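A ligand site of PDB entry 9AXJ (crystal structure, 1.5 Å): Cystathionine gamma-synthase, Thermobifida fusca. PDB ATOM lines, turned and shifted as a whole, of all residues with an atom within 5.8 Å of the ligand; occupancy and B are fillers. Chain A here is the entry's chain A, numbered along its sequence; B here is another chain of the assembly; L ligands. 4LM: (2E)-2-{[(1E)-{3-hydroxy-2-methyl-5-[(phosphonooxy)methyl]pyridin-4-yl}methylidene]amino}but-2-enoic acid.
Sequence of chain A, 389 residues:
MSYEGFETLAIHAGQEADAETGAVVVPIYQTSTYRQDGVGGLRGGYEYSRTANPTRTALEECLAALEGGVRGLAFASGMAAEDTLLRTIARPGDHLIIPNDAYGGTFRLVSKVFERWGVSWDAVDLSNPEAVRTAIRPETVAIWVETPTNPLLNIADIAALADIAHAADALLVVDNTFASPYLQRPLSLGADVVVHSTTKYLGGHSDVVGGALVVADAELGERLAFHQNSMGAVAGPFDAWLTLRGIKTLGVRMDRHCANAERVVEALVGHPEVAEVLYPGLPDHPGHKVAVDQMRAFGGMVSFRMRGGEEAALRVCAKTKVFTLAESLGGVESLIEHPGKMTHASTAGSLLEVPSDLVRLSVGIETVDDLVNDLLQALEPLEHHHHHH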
ATOM      1  N   SER A  77      11.231   9.676  16.389  1.00  0.00           N
ATOM      2  CA  SER A  77       9.788   9.487  16.270  1.00  0.00           C
ATOM      3  C   SER A  77       9.328  10.202  14.975  1.00  0.00           C
ATOM      4  O   SER A  77      10.076  11.026  14.446  1.00  0.00           O
ATOM      5  CB  SER A  77       9.026  10.044  17.438  1.00  0.00           C
ATOM      6  OG  SER A  77       9.187  11.470  17.546  1.00  0.00           O
ATOM      7  N   GLY A  78       8.123   9.924  14.511  1.00  0.00           N
ATOM      8  CA  GLY A  78       7.481  10.703  13.455  1.00  0.00           C
ATOM      9  C   GLY A  78       7.475  12.187  13.817  1.00  0.00           C
ATOM     10  O   GLY A  78       7.801  13.035  12.963  1.00  0.00           O
ATOM     11  N   MET A  79       7.069  12.492  15.048  1.00  0.00           N
ATOM     12  CA  MET A  79       6.981  13.896  15.462  1.00  0.00           C
ATOM     13  C   MET A  79       8.367  14.541  15.409  1.00  0.00           C
ATOM     14  O   MET A  79       8.477  15.734  14.990  1.00  0.00           O
ATOM     15  CB  MET A  79       6.381  14.081  16.826  1.00  0.00           C
ATOM     16  CG  MET A  79       4.901  13.766  16.869  1.00  0.00           C
ATOM     17  SD  MET A  79       3.885  14.542  15.590  1.00  0.00           S
ATOM     18  CE  MET A  79       4.507  16.227  15.609  1.00  0.00           C
ATOM     19  N   ALA A  80       9.440  13.828  15.740  1.00  0.00           N
ATOM     20  CA  ALA A  80      10.772  14.421  15.680  1.00  0.00           C
ATOM     21  C   ALA A  80      11.228  14.660  14.239  1.00  0.00           C
ATOM     22  O   ALA A  80      11.875  15.693  13.931  1.00  0.00           O
ATOM     23  CB  ALA A  80      11.792  13.548  16.385  1.00  0.00           C
ATOM     24  N   GLU A  82       9.078  15.508  11.861  1.00  0.00           N
ATOM     25  CA  GLU A  82       8.301  16.715  11.559  1.00  0.00           C
ATOM     26  C   GLU A  82       9.013  17.926  12.145  1.00  0.00           C
ATOM     27  O   GLU A  82       9.150  18.971  11.468  1.00  0.00           O
ATOM     28  CB  GLU A  82       6.897  16.666  12.113  1.00  0.00           C
ATOM     29  CG  GLU A  82       5.991  15.571  11.586  1.00  0.00           C
ATOM     30  CD  GLU A  82       4.513  15.770  11.964  1.00  0.00           C
ATOM     31  OE1 GLU A  82       4.153  16.824  12.512  1.00  0.00           O
ATOM     32  OE2 GLU A  82       3.779  14.847  11.683  1.00  0.00           O
ATOM     33  N   TYR A 103      -3.222  14.188  11.540  1.00  0.00           N
ATOM     34  CA  TYR A 103      -2.837  13.626  12.850  1.00  0.00           C
ATOM     35  C   TYR A 103      -2.839  14.762  13.904  1.00  0.00           C
ATOM     36  O   TYR A 103      -2.234  15.822  13.689  1.00  0.00           O
ATOM     37  CB  TYR A 103      -1.448  12.916  12.811  1.00  0.00           C
ATOM     38  CG  TYR A 103      -1.000  12.487  14.174  1.00  0.00           C
ATOM     39  CD1 TYR A 103      -1.860  11.839  15.048  1.00  0.00           C
ATOM     40  CD2 TYR A 103       0.221  12.854  14.664  1.00  0.00           C
ATOM     41  CE1 TYR A 103      -1.486  11.511  16.362  1.00  0.00           C
ATOM     42  CE2 TYR A 103       0.646  12.500  15.943  1.00  0.00           C
ATOM     43  CZ  TYR A 103      -0.243  11.888  16.817  1.00  0.00           C
ATOM     44  OH  TYR A 103       0.116  11.630  18.134  1.00  0.00           O
ATOM     45  N   THR A 106       0.524  16.461  14.662  1.00  0.00           N
ATOM     46  CA  THR A 106       0.962  17.421  13.654  1.00  0.00           C
ATOM     47  C   THR A 106       0.346  18.784  13.986  1.00  0.00           C
ATOM     48  O   THR A 106       1.041  19.815  14.012  1.00  0.00           O
ATOM     49  CB  THR A 106       0.585  16.972  12.250  1.00  0.00           C
ATOM     50  OG1 THR A 106       1.197  15.696  12.028  1.00  0.00           O
ATOM     51  CG2 THR A 106       1.122  17.949  11.235  1.00  0.00           C
ATOM     52  N   GLU A 146      -1.261  15.465   4.121  1.00  0.00           N
ATOM     53  CA  GLU A 146      -1.458  14.024   4.435  1.00  0.00           C
ATOM     54  C   GLU A 146      -2.403  13.516   3.347  1.00  0.00           C
ATOM     55  O   GLU A 146      -3.440  14.165   3.085  1.00  0.00           O
ATOM     56  CB  GLU A 146      -2.155  13.797   5.779  1.00  0.00           C
ATOM     57  CG  GLU A 146      -1.320  13.984   6.992  1.00  0.00           C
ATOM     58  CD  GLU A 146      -1.989  13.698   8.317  1.00  0.00           C
ATOM     59  OE1 GLU A 146      -3.011  12.989   8.315  1.00  0.00           O
ATOM     60  OE2 GLU A 146      -1.440  14.105   9.365  1.00  0.00           O
ATOM     61  N   ASN A 150      -5.545  11.505   8.272  1.00  0.00           N
ATOM     62  CA  ASN A 150      -5.788  10.807   9.544  1.00  0.00           C
ATOM     63  C   ASN A 150      -6.787  11.634  10.345  1.00  0.00           C
ATOM     64  O   ASN A 150      -6.437  12.756  10.791  1.00  0.00           O
ATOM     65  CB  ASN A 150      -4.477  10.633  10.286  1.00  0.00           C
ATOM     66  CG  ASN A 150      -4.614   9.932  11.605  1.00  0.00           C
ATOM     67  OD1 ASN A 150      -5.716   9.545  11.997  1.00  0.00           O
ATOM     68  ND2 ASN A 150      -3.459   9.817  12.324  1.00  0.00           N
ATOM     69  N   ASP A 175       3.238  13.756   4.053  1.00  0.00           N
ATOM     70  CA  ASP A 175       3.266  12.750   5.128  1.00  0.00           C
ATOM     71  C   ASP A 175       2.622  11.490   4.542  1.00  0.00           C
ATOM     72  O   ASP A 175       1.393  11.462   4.329  1.00  0.00           O
ATOM     73  CB  ASP A 175       2.577  13.272   6.380  1.00  0.00           C
ATOM     74  CG  ASP A 175       2.643  12.299   7.548  1.00  0.00           C
ATOM     75  OD1 ASP A 175       2.765  11.092   7.311  1.00  0.00           O
ATOM     76  OD2 ASP A 175       2.505  12.810   8.720  1.00  0.00           O
ATOM     77  N   THR A 177       2.764   8.411   5.708  1.00  0.00           N
ATOM     78  CA  THR A 177       2.662   7.410   6.769  1.00  0.00           C
ATOM     79  C   THR A 177       1.578   6.367   6.469  1.00  0.00           C
ATOM     80  O   THR A 177       1.895   5.142   6.476  1.00  0.00           O
ATOM     81  CB  THR A 177       2.374   8.055   8.132  1.00  0.00           C
ATOM     82  OG1 THR A 177       3.465   8.903   8.488  1.00  0.00           O
ATOM     83  CG2 THR A 177       2.135   7.044   9.231  1.00  0.00           C
ATOM     84  N   PHE A 178       0.359   6.789   6.162  1.00  0.00           N
ATOM     85  CA  PHE A 178      -0.785   5.848   5.999  1.00  0.00           C
ATOM     86  C   PHE A 178      -0.587   4.997   4.748  1.00  0.00           C
ATOM     87  O   PHE A 178      -0.894   3.812   4.781  1.00  0.00           O
ATOM     88  CB  PHE A 178      -2.087   6.630   5.930  1.00  0.00           C
ATOM     89  CG  PHE A 178      -2.717   6.931   7.282  1.00  0.00           C
ATOM     90  CD1 PHE A 178      -1.972   7.241   8.398  1.00  0.00           C
ATOM     91  CD2 PHE A 178      -4.072   6.953   7.358  1.00  0.00           C
ATOM     92  CE1 PHE A 178      -2.608   7.471   9.630  1.00  0.00           C
ATOM     93  CE2 PHE A 178      -4.729   7.147   8.579  1.00  0.00           C
ATOM     94  CZ  PHE A 178      -3.976   7.410   9.716  1.00  0.00           C
ATOM     95  N   VAL A 195       7.543  12.646   4.588  1.00  0.00           N
ATOM     96  CA  VAL A 195       7.598  12.380   6.027  1.00  0.00           C
ATOM     97  C   VAL A 195       6.978  11.048   6.298  1.00  0.00           C
ATOM     98  O   VAL A 195       5.898  10.760   5.748  1.00  0.00           O
ATOM     99  CB  VAL A 195       6.843  13.477   6.810  1.00  0.00           C
ATOM    100  CG1 VAL A 195       6.767  13.164   8.305  1.00  0.00           C
ATOM    101  CG2 VAL A 195       7.436  14.829   6.568  1.00  0.00           C
ATOM    102  N   HIS A 196       7.566  10.269   7.213  1.00  0.00           N
ATOM    103  CA  HIS A 196       6.910   9.078   7.778  1.00  0.00           C
ATOM    104  C   HIS A 196       7.012   9.066   9.273  1.00  0.00           C
ATOM    105  O   HIS A 196       8.099   9.362   9.802  1.00  0.00           O
ATOM    106  CB  HIS A 196       7.579   7.786   7.313  1.00  0.00           C
ATOM    107  CG  HIS A 196       7.374   7.460   5.888  1.00  0.00           C
ATOM    108  ND1 HIS A 196       6.212   6.886   5.453  1.00  0.00           N
ATOM    109  CD2 HIS A 196       8.176   7.643   4.804  1.00  0.00           C
ATOM    110  CE1 HIS A 196       6.295   6.735   4.148  1.00  0.00           C
ATOM    111  NE2 HIS A 196       7.487   7.225   3.715  1.00  0.00           N
ATOM    112  N   SER A 197       5.939   8.622   9.927  1.00  0.00           N
ATOM    113  CA  SER A 197       6.053   7.902  11.216  1.00  0.00           C
ATOM    114  C   SER A 197       6.404   6.472  10.845  1.00  0.00           C
ATOM    115  O   SER A 197       5.549   5.761  10.345  1.00  0.00           O
ATOM    116  CB  SER A 197       4.786   7.928  11.953  1.00  0.00           C
ATOM    117  OG  SER A 197       4.897   7.128  13.123  1.00  0.00           O
ATOM    118  N   THR A 198       7.647   6.053  11.011  1.00  0.00           N
ATOM    119  CA  THR A 198       8.033   4.643  10.792  1.00  0.00           C
ATOM    120  C   THR A 198       7.439   3.746  11.869  1.00  0.00           C
ATOM    121  O   THR A 198       7.489   2.524  11.684  1.00  0.00           O
ATOM    122  CB  THR A 198       9.541   4.510  10.610  1.00  0.00           C
ATOM    123  OG1 THR A 198      10.165   4.875  11.835  1.00  0.00           O
ATOM    124  CG2 THR A 198      10.080   5.336   9.479  1.00  0.00           C
ATOM    125  N   THR A 199       6.874   4.309  12.899  1.00  0.00           N
ATOM    126  CA  THR A 199       6.191   3.579  13.959  1.00  0.00           C
ATOM    127  C   THR A 199       5.082   2.739  13.335  1.00  0.00           C
ATOM    128  O   THR A 199       4.616   1.775  13.939  1.00  0.00           O
ATOM    129  CB  THR A 199       5.622   4.576  14.938  1.00  0.00           C
ATOM    130  OG1 THR A 199       6.601   5.524  15.356  1.00  0.00           O
ATOM    131  CG2 THR A 199       5.001   3.917  16.124  1.00  0.00           C
ATOM    132  N   LYS A 200       4.528   3.207  12.221  1.00  0.00           N
ATOM    133  CA  LYS A 200       3.275   2.628  11.663  1.00  0.00           C
ATOM    134  C   LYS A 200       3.646   1.493  10.704  1.00  0.00           C
ATOM    135  O   LYS A 200       4.252   0.512  11.145  1.00  0.00           O
ATOM    136  CB  LYS A 200       2.397   3.754  11.097  1.00  0.00           C
ATOM    137  CG  LYS A 200       2.246   4.965  12.011  1.00  0.00           C
ATOM    138  CD  LYS A 200       1.972   4.646  13.445  1.00  0.00           C
ATOM    139  CE  LYS A 200       1.651   5.881  14.253  1.00  0.00           C
ATOM    140  NZ  LYS A 200       1.707   5.607  15.707  1.00  0.00           N
ATOM    141  N   VAL A 209       9.055   3.137  17.996  1.00  0.00           N
ATOM    142  CA  VAL A 209       8.654   4.509  17.638  1.00  0.00           C
ATOM    143  C   VAL A 209       9.815   5.096  16.867  1.00  0.00           C
ATOM    144  O   VAL A 209      10.929   5.094  17.359  1.00  0.00           O
ATOM    145  CB  VAL A 209       8.276   5.285  18.888  1.00  0.00           C
ATOM    146  CG1 VAL A 209       8.149   6.774  18.614  1.00  0.00           C
ATOM    147  CG2 VAL A 209       6.997   4.751  19.540  1.00  0.00           C
ATOM    148  N   GLY A 210       9.503   5.667  15.721  1.00  0.00           N
ATOM    149  CA  GLY A 210      10.526   6.248  14.880  1.00  0.00           C
ATOM    150  C   GLY A 210       9.929   7.101  13.789  1.00  0.00           C
ATOM    151  O   GLY A 210       8.726   6.990  13.540  1.00  0.00           O
ATOM    152  N   GLY A 211      10.775   7.933  13.191  1.00  0.00           N
ATOM    153  CA  GLY A 211      10.367   8.796  12.061  1.00  0.00           C
ATOM    154  C   GLY A 211      11.381   8.800  10.951  1.00  0.00           C
ATOM    155  O   GLY A 211      12.552   8.371  11.139  1.00  0.00           O
ATOM    156  N   GLU A 327      -4.094   3.586  20.840  1.00  0.00           N
ATOM    157  CA  GLU A 327      -3.567   4.500  19.826  1.00  0.00           C
ATOM    158  C   GLU A 327      -2.652   3.715  18.867  1.00  0.00           C
ATOM    159  O   GLU A 327      -2.264   2.545  19.147  1.00  0.00           O
ATOM    160  CB  GLU A 327      -2.868   5.671  20.501  1.00  0.00           C
ATOM    161  CG  GLU A 327      -3.823   6.528  21.309  1.00  0.00           C
ATOM    162  CD  GLU A 327      -3.340   7.954  21.564  1.00  0.00           C
ATOM    163  OE1 GLU A 327      -2.111   8.293  21.241  1.00  0.00           O
ATOM    164  OE2 GLU A 327      -4.115   8.704  22.189  1.00  0.00           O
ATOM    165  N   SER A 328      -2.310   4.357  17.784  1.00  0.00           N
ATOM    166  CA  SER A 328      -1.382   3.847  16.784  1.00  0.00           C
ATOM    167  C   SER A 328      -2.064   3.037  15.690  1.00  0.00           C
ATOM    168  O   SER A 328      -3.330   2.906  15.659  1.00  0.00           O
ATOM    169  CB  SER A 328      -0.220   3.090  17.402  1.00  0.00           C
ATOM    170  OG  SER A 328       0.867   3.110  16.440  1.00  0.00           O
ATOM    171  N   LEU A 329      -1.287   2.624  14.704  1.00  0.00           N
ATOM    172  CA  LEU A 329      -1.826   1.977  13.481  1.00  0.00           C
ATOM    173  C   LEU A 329      -0.663   1.315  12.747  1.00  0.00           C
ATOM    174  O   LEU A 329       0.507   1.549  13.105  1.00  0.00           O
ATOM    175  CB  LEU A 329      -2.526   3.017  12.593  1.00  0.00           C
ATOM    176  CG  LEU A 329      -1.611   4.154  12.097  1.00  0.00           C
ATOM    177  CD1 LEU A 329      -1.467   4.177  10.567  1.00  0.00           C
ATOM    178  CD2 LEU A 329      -2.030   5.472  12.626  1.00  0.00           C
ATOM    179  N   GLU A 337      -9.724   2.621  17.636  1.00  0.00           N
ATOM    180  CA  GLU A 337      -9.731   3.757  18.560  1.00  0.00           C
ATOM    181  C   GLU A 337     -10.868   4.717  18.233  1.00  0.00           C
ATOM    182  O   GLU A 337     -11.508   4.613  17.193  1.00  0.00           O
ATOM    183  CB  GLU A 337      -8.398   4.543  18.547  1.00  0.00           C
ATOM    184  CG  GLU A 337      -8.117   5.243  17.242  1.00  0.00           C
ATOM    185  CD  GLU A 337      -7.666   6.695  17.368  1.00  0.00           C
ATOM    186  OE1 GLU A 337      -7.421   7.375  16.314  1.00  0.00           O
ATOM    187  OE2 GLU A 337      -7.492   7.178  18.504  1.00  0.00           O
ATOM    188  N   THR A 343      -6.478   9.898  19.709  1.00  0.00           N
ATOM    189  CA  THR A 343      -5.389  10.522  18.933  1.00  0.00           C
ATOM    190  C   THR A 343      -5.701  11.986  18.593  1.00  0.00           C
ATOM    191  O   THR A 343      -4.738  12.708  18.279  1.00  0.00           O
ATOM    192  CB  THR A 343      -5.191   9.771  17.597  1.00  0.00           C
ATOM    193  OG1 THR A 343      -6.423   9.648  16.895  1.00  0.00           O
ATOM    194  CG2 THR A 343      -4.552   8.433  17.881  1.00  0.00           C
ATOM    195  N   HIS A 344      -6.970  12.346  18.547  1.00  0.00           N
ATOM    196  CA  HIS A 344      -7.358  13.694  18.079  1.00  0.00           C
ATOM    197  C   HIS A 344      -8.068  14.486  19.172  1.00  0.00           C
ATOM    198  O   HIS A 344      -8.706  15.529  18.913  1.00  0.00           O
ATOM    199  CB  HIS A 344      -8.189  13.621  16.801  1.00  0.00           C
ATOM    200  CG  HIS A 344      -7.430  13.162  15.605  1.00  0.00           C
ATOM    201  ND1 HIS A 344      -6.990  11.838  15.487  1.00  0.00           N
ATOM    202  CD2 HIS A 344      -7.030  13.817  14.469  1.00  0.00           C
ATOM    203  CE1 HIS A 344      -6.319  11.730  14.336  1.00  0.00           C
ATOM    204  NE2 HIS A 344      -6.398  12.949  13.651  1.00  0.00           N
ATOM    205  N   ARG A 360     -12.072   4.673  14.276  1.00  0.00           N
ATOM    206  CA  ARG A 360     -10.984   4.435  13.313  1.00  0.00           C
ATOM    207  C   ARG A 360     -10.480   2.998  13.525  1.00  0.00           C
ATOM    208  O   ARG A 360     -10.157   2.650  14.700  1.00  0.00           O
ATOM    209  CB  ARG A 360      -9.819   5.420  13.472  1.00  0.00           C
ATOM    210  CG  ARG A 360      -8.816   5.323  12.388  1.00  0.00           C
ATOM    211  CD  ARG A 360      -7.610   6.201  12.665  1.00  0.00           C
ATOM    212  NE  ARG A 360      -6.771   5.536  13.683  1.00  0.00           N
ATOM    213  CZ  ARG A 360      -5.690   6.111  14.225  1.00  0.00           C
ATOM    214  NH1 ARG A 360      -5.260   7.318  13.843  1.00  0.00           N
ATOM    215  NH2 ARG A 360      -4.944   5.427  15.099  1.00  0.00           N
ATOM    216  N   TYR B  48       0.886   5.701  24.909  1.00  0.00           N
ATOM    217  CA  TYR B  48       1.649   5.716  23.643  1.00  0.00           C
ATOM    218  C   TYR B  48       3.100   5.993  23.996  1.00  0.00           C
ATOM    219  O   TYR B  48       3.375   6.934  24.773  1.00  0.00           O
ATOM    220  CB  TYR B  48       1.090   6.770  22.673  1.00  0.00           C
ATOM    221  CG  TYR B  48       1.763   6.748  21.346  1.00  0.00           C
ATOM    222  CD1 TYR B  48       1.585   5.640  20.500  1.00  0.00           C
ATOM    223  CD2 TYR B  48       2.581   7.758  20.943  1.00  0.00           C
ATOM    224  CE1 TYR B  48       2.284   5.543  19.321  1.00  0.00           C
ATOM    225  CE2 TYR B  48       3.253   7.709  19.706  1.00  0.00           C
ATOM    226  CZ  TYR B  48       3.072   6.604  18.887  1.00  0.00           C
ATOM    227  OH  TYR B  48       3.748   6.568  17.670  1.00  0.00           O
ATOM    228  N   ARG B  50       5.813   7.427  22.730  1.00  0.00           N
ATOM    229  CA  ARG B  50       6.395   8.795  22.680  1.00  0.00           C
ATOM    230  C   ARG B  50       6.008   9.572  23.950  1.00  0.00           C
ATOM    231  O   ARG B  50       6.842  10.242  24.547  1.00  0.00           O
ATOM    232  CB  ARG B  50       5.934   9.504  21.414  1.00  0.00           C
ATOM    233  CG  ARG B  50       6.392  10.951  21.362  1.00  0.00           C
ATOM    234  CD  ARG B  50       6.300  11.533  19.950  1.00  0.00           C
ATOM    235  NE  ARG B  50       5.197  11.137  19.118  1.00  0.00           N
ATOM    236  CZ  ARG B  50       3.921  11.393  19.350  1.00  0.00           C
ATOM    237  NH1 ARG B  50       2.993  10.910  18.546  1.00  0.00           N
ATOM    238  NH2 ARG B  50       3.550  12.138  20.390  1.00  0.00           N
HETATM  239  C   4LM L   1      -2.041   7.613  15.568  1.00  0.00           C
HETATM  240  N   4LM L   1      -0.210   8.793  14.685  1.00  0.00           N
HETATM  241  O1  4LM L   1      -2.776   8.249  14.779  1.00  0.00           O
HETATM  242  P   4LM L   1       5.034   9.313  15.902  1.00  0.00           P
HETATM  243  N1  4LM L   1       2.064  11.426  11.009  1.00  0.00           N
HETATM  244  C2  4LM L   1       0.892  10.717  10.986  1.00  0.00           C
HETATM  245  C3  4LM L   1       0.509  10.037  12.141  1.00  0.00           C
HETATM  246  O3  4LM L   1      -0.601   9.423  12.197  1.00  0.00           O
HETATM  247  C4  4LM L   1       1.376  10.048  13.302  1.00  0.00           C
HETATM  248  C5  4LM L   1       2.579  10.780  13.239  1.00  0.00           C
HETATM  249  C6  4LM L   1       2.879  11.475  12.081  1.00  0.00           C
HETATM  250  CA  4LM L   1      -0.729   8.106  15.756  1.00  0.00           C
HETATM  251  CB  4LM L   1       0.083   8.140  17.008  1.00  0.00           C
HETATM  252  CG  4LM L   1      -0.459   7.802  18.310  1.00  0.00           C
HETATM  253  C2A 4LM L   1       0.044  10.717   9.739  1.00  0.00           C
HETATM  254  C4A 4LM L   1       0.990   9.326  14.527  1.00  0.00           C
HETATM  255  C5A 4LM L   1       3.498  10.918  14.424  1.00  0.00           C
HETATM  256  OP1 4LM L   1       3.865   8.866  16.797  1.00  0.00           O
HETATM  257  OP2 4LM L   1       5.766  10.496  16.478  1.00  0.00           O
HETATM  258  OP3 4LM L   1       5.988   8.174  15.474  1.00  0.00           O
HETATM  259  OP4 4LM L   1       4.399   9.798  14.462  1.00  0.00           O
HETATM  260  O2  4LM L   1      -2.485   6.691  16.154  1.00  0.00           O
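The side-chain hydroxyl of Thr 199 sits at hydrogen-bond distance from the backbone NH of Gly 210 (2.9 Å). NH1 of Arg 50 of chain B lies within hydrogen-bond range of OH of Tyr 103, at 3.0 Å. The guanidinium group of Arg 360 is in hydrogen-bond range of the backbone carbonyl oxygen of Ser 328 (3.0 Å). The side-chain amide oxygen (OD1) of Asn 150 sits at hydrogen-bond distance from the guanidinium group (NH1) of Arg 360, at 2.9 Å. OG of Ser 328 sits at hydrogen-bond distance from NZ of Lys 200 (2.7 Å). The side-chain carboxylate of Glu 146 sits at hydrogen-bond distance from the backbone NH of Asn 150. A ring nitrogen (NE2) of His 344 is in hydrogen-bond range of the backbone carbonyl oxygen (O) of Asn 150 (2.9 Å). The side-chain hydroxyl (OG1) of Thr 343 is in hydrogen-bond range of a ring nitrogen (ND1) of His 344 (2.7 Å).
The side-chain hydroxyl of Tyr 48 of chain B lies within hydrogen-bond range of an oxygen (OP1) of the ligand. N1 of the ligand is in hydrogen-bond range of OD2 of Asp 175, 2.7 Å away. The side-chain hydroxyl of Thr 199 is in hydrogen-bond range of an oxygen (OP3) of the ligand (2.7 Å). The guanidinium group (NE) of Arg 50 of chain B lies within salt-bridge range of an oxygen (OP2) of the ligand. OP2 of the ligand is in hydrogen-bond range of N of Met 79 (2.8 Å). OG of Ser 197 lies within hydrogen-bond range of OP3 of the ligand (2.8 Å). The guanidinium group (NH1) of Arg 360 lies within salt-bridge range of an oxygen (O1) of the ligand (2.8 Å). An oxygen (O2) of the ligand sits at hydrogen-bond distance from the backbone NH (N) of Ser 328 (2.9 Å). O3 of the ligand lies within hydrogen-bond range of ND2 of Asn 150. An oxygen (OP3) of the ligand lies within hydrogen-bond range of the backbone NH of Gly 78 (2.9 Å).
Merely in contact with the ligand: Thr 343 (3.2 Å), Lys 200 (3.3 Å), Tyr 103 (3.3 Å), Glu 327 (3.4 Å), Ser 77 (3.4 Å), Glu 82 (3.5 Å), Gly 210 (3.6 Å), Leu 329 (3.6 Å), Glu 146 (3.7 Å), Phe 178 (3.8 Å) and Thr 177 (3.8 Å). Within 4 Å of the ligand: Ser 77, Gly 78, Met 79, Glu 82, Tyr 103, Glu 146, Asn 150, Asp 175, Thr 177, Phe 178, Ser 197, Thr 199, Lys 200, Gly 210, Glu 327, Ser 328, Leu 329, Thr 343, Arg 360, Tyr 48 of chain B and Arg 50 of chain B. The nearest printed residue that does not touch the ligand is Val 209 (4.1 Å).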
